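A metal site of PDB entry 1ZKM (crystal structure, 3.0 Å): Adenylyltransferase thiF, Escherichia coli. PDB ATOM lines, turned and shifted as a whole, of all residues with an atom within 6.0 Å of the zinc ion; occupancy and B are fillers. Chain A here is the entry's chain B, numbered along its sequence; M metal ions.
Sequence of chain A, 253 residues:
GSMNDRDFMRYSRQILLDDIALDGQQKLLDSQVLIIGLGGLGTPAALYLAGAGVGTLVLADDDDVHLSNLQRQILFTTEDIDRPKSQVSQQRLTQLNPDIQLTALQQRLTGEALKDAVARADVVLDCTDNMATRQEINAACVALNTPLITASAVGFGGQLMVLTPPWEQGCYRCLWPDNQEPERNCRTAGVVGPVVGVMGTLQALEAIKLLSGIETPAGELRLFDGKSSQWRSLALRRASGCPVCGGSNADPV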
ATOM      1  N   ASN A 138     -28.904 -32.306  -3.434  1.00  0.00           N
ATOM      2  CA  ASN A 138     -28.196 -31.124  -3.943  1.00  0.00           C
ATOM      3  C   ASN A 138     -27.400 -30.477  -2.813  1.00  0.00           C
ATOM      4  O   ASN A 138     -26.318 -29.943  -3.036  1.00  0.00           O
ATOM      5  CB  ASN A 138     -29.189 -30.090  -4.502  1.00  0.00           C
ATOM      6  CG  ASN A 138     -28.484 -28.852  -5.099  1.00  0.00           C
ATOM      7  OD1 ASN A 138     -27.913 -28.914  -6.183  1.00  0.00           O
ATOM      8  ND2 ASN A 138     -28.522 -27.744  -4.371  1.00  0.00           N
ATOM      9  N   GLY A 170     -24.467 -22.305 -10.399  1.00  0.00           N
ATOM     10  CA  GLY A 170     -25.520 -22.673  -9.467  1.00  0.00           C
ATOM     11  C   GLY A 170     -25.607 -24.100  -8.965  1.00  0.00           C
ATOM     12  O   GLY A 170     -24.853 -24.978  -9.398  1.00  0.00           O
ATOM     13  N   CYS A 171     -26.526 -24.303  -8.024  1.00  0.00           N
ATOM     14  CA  CYS A 171     -26.790 -25.600  -7.419  1.00  0.00           C
ATOM     15  C   CYS A 171     -28.249 -25.829  -7.805  1.00  0.00           C
ATOM     16  O   CYS A 171     -28.789 -25.053  -8.588  1.00  0.00           O
ATOM     17  CB  CYS A 171     -26.680 -25.538  -5.899  1.00  0.00           C
ATOM     18  SG  CYS A 171     -28.063 -24.656  -5.124  1.00  0.00           S
ATOM     19  N   TYR A 172     -28.885 -26.867  -7.259  1.00  0.00           N
ATOM     20  CA  TYR A 172     -30.281 -27.120  -7.616  1.00  0.00           C
ATOM     21  C   TYR A 172     -31.241 -26.161  -6.948  1.00  0.00           C
ATOM     22  O   TYR A 172     -32.373 -26.004  -7.392  1.00  0.00           O
ATOM     23  CB  TYR A 172     -30.694 -28.559  -7.301  1.00  0.00           C
ATOM     24  CG  TYR A 172     -32.037 -28.907  -7.883  1.00  0.00           C
ATOM     25  CD1 TYR A 172     -32.226 -28.954  -9.259  1.00  0.00           C
ATOM     26  CD2 TYR A 172     -33.145 -29.131  -7.068  1.00  0.00           C
ATOM     27  CE1 TYR A 172     -33.483 -29.213  -9.815  1.00  0.00           C
ATOM     28  CE2 TYR A 172     -34.411 -29.384  -7.604  1.00  0.00           C
ATOM     29  CZ  TYR A 172     -34.570 -29.425  -8.984  1.00  0.00           C
ATOM     30  OH  TYR A 172     -35.812 -29.646  -9.549  1.00  0.00           O
ATOM     31  N   ARG A 173     -30.812 -25.535  -5.867  1.00  0.00           N
ATOM     32  CA  ARG A 173     -31.670 -24.577  -5.173  1.00  0.00           C
ATOM     33  C   ARG A 173     -31.552 -23.256  -5.903  1.00  0.00           C
ATOM     34  O   ARG A 173     -32.547 -22.533  -6.043  1.00  0.00           O
ATOM     35  CB  ARG A 173     -31.233 -24.429  -3.729  1.00  0.00           C
ATOM     36  CG  ARG A 173     -31.670 -25.597  -2.883  1.00  0.00           C
ATOM     37  CD  ARG A 173     -30.735 -25.839  -1.738  1.00  0.00           C
ATOM     38  NE  ARG A 173     -31.137 -27.018  -0.985  1.00  0.00           N
ATOM     39  CZ  ARG A 173     -30.406 -27.564  -0.017  1.00  0.00           C
ATOM     40  NH1 ARG A 173     -29.234 -27.032   0.312  1.00  0.00           N
ATOM     41  NH2 ARG A 173     -30.858 -28.636   0.618  1.00  0.00           N
ATOM     42  N   CYS A 174     -30.354 -22.936  -6.373  1.00  0.00           N
ATOM     43  CA  CYS A 174     -30.143 -21.716  -7.137  1.00  0.00           C
ATOM     44  C   CYS A 174     -31.131 -21.626  -8.249  1.00  0.00           C
ATOM     45  O   CYS A 174     -31.286 -20.572  -8.869  1.00  0.00           O
ATOM     46  CB  CYS A 174     -28.815 -21.720  -7.823  1.00  0.00           C
ATOM     47  SG  CYS A 174     -27.511 -21.309  -6.692  1.00  0.00           S
ATOM     48  N   ARG A 238     -26.038 -19.144 -10.950  1.00  0.00           N
ATOM     49  CA  ARG A 238     -25.997 -19.310  -9.507  1.00  0.00           C
ATOM     50  C   ARG A 238     -26.701 -18.120  -8.867  1.00  0.00           C
ATOM     51  O   ARG A 238     -26.254 -16.983  -8.982  1.00  0.00           O
ATOM     52  CB  ARG A 238     -24.560 -19.389  -9.010  1.00  0.00           C
ATOM     53  CG  ARG A 238     -23.671 -18.289  -9.526  1.00  0.00           C
ATOM     54  CD  ARG A 238     -22.393 -18.232  -8.722  1.00  0.00           C
ATOM     55  NE  ARG A 238     -21.590 -17.067  -9.088  1.00  0.00           N
ATOM     56  CZ  ARG A 238     -20.693 -16.511  -8.290  1.00  0.00           C
ATOM     57  NH1 ARG A 238     -20.480 -17.004  -7.075  1.00  0.00           N
ATOM     58  NH2 ARG A 238     -20.001 -15.456  -8.698  1.00  0.00           N
ATOM     59  N   ALA A 239     -27.818 -18.401  -8.206  1.00  0.00           N
ATOM     60  CA  ALA A 239     -28.624 -17.371  -7.555  1.00  0.00           C
ATOM     61  C   ALA A 239     -27.825 -16.521  -6.568  1.00  0.00           C
ATOM     62  O   ALA A 239     -26.943 -17.024  -5.861  1.00  0.00           O
ATOM     63  CB  ALA A 239     -29.804 -18.007  -6.858  1.00  0.00           C
ATOM     64  N   CYS A 242     -27.266 -17.739  -2.743  1.00  0.00           N
ATOM     65  CA  CYS A 242     -27.912 -19.027  -2.643  1.00  0.00           C
ATOM     66  C   CYS A 242     -27.563 -19.735  -1.332  1.00  0.00           C
ATOM     67  O   CYS A 242     -26.388 -19.804  -0.957  1.00  0.00           O
ATOM     68  CB  CYS A 242     -27.519 -19.936  -3.783  1.00  0.00           C
ATOM     69  SG  CYS A 242     -28.236 -21.546  -3.479  1.00  0.00           S
ATOM     70  N   PRO A 243     -28.571 -20.274  -0.630  1.00  0.00           N
ATOM     71  CA  PRO A 243     -28.391 -20.989   0.644  1.00  0.00           C
ATOM     72  C   PRO A 243     -27.468 -22.219   0.615  1.00  0.00           C
ATOM     73  O   PRO A 243     -27.534 -23.056   1.506  1.00  0.00           O
ATOM     74  CB  PRO A 243     -29.823 -21.361   1.029  1.00  0.00           C
ATOM     75  CG  PRO A 243     -30.631 -20.239   0.441  1.00  0.00           C
ATOM     76  CD  PRO A 243     -30.000 -20.054  -0.912  1.00  0.00           C
ATOM     77  N   VAL A 244     -26.622 -22.312  -0.408  1.00  0.00           N
ATOM     78  CA  VAL A 244     -25.688 -23.435  -0.529  1.00  0.00           C
ATOM     79  C   VAL A 244     -24.431 -22.971  -1.262  1.00  0.00           C
ATOM     80  O   VAL A 244     -23.313 -23.143  -0.768  1.00  0.00           O
ATOM     81  CB  VAL A 244     -26.294 -24.644  -1.281  1.00  0.00           C
ATOM     82  CG1 VAL A 244     -26.181 -25.887  -0.433  1.00  0.00           C
ATOM     83  CG2 VAL A 244     -27.751 -24.364  -1.648  1.00  0.00           C
ATOM     84  N   CYS A 245     -24.603 -22.410  -2.456  1.00  0.00           N
ATOM     85  CA  CYS A 245     -23.445 -21.912  -3.183  1.00  0.00           C
ATOM     86  C   CYS A 245     -22.885 -20.723  -2.459  1.00  0.00           C
ATOM     87  O   CYS A 245     -23.271 -19.608  -2.824  1.00  0.00           O
ATOM     88  CB  CYS A 245     -23.836 -21.378  -4.558  1.00  0.00           C
ATOM     89  SG  CYS A 245     -24.358 -22.759  -5.562  1.00  0.00           S
HETATM   90 ZN    ZN M   1     -26.797 -22.565  -5.002  1.00  0.00          ZN
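The side-chain sulfur of Cys 174 lies close to the backbone NH of Ala 239 (3.3 Å).
N of Val 244 sits close to SG of Cys 242, at 3.6 Å.
The backbone NH (N) of Arg 173 lies close to the side-chain sulfur (SG) of Cys 171, at 3.0 Å.
The side-chain sulfur of Cys 171 sits close to the side-chain amide nitrogen of Asn 138 (3.2 Å).
Val 244 touches the zinc ion.
Of the 12 residues printed, 5 come within 4 Å of the zinc ion.
Along chain A the residues within 4 Å of the zinc ion span positions 171 to 245.
The zinc ion is bound by the side-chain sulfur of Cys 174, the side-chain sulfur of Cys 242, the side-chain sulfur of Cys 171 and the side-chain sulfur of Cys 245.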
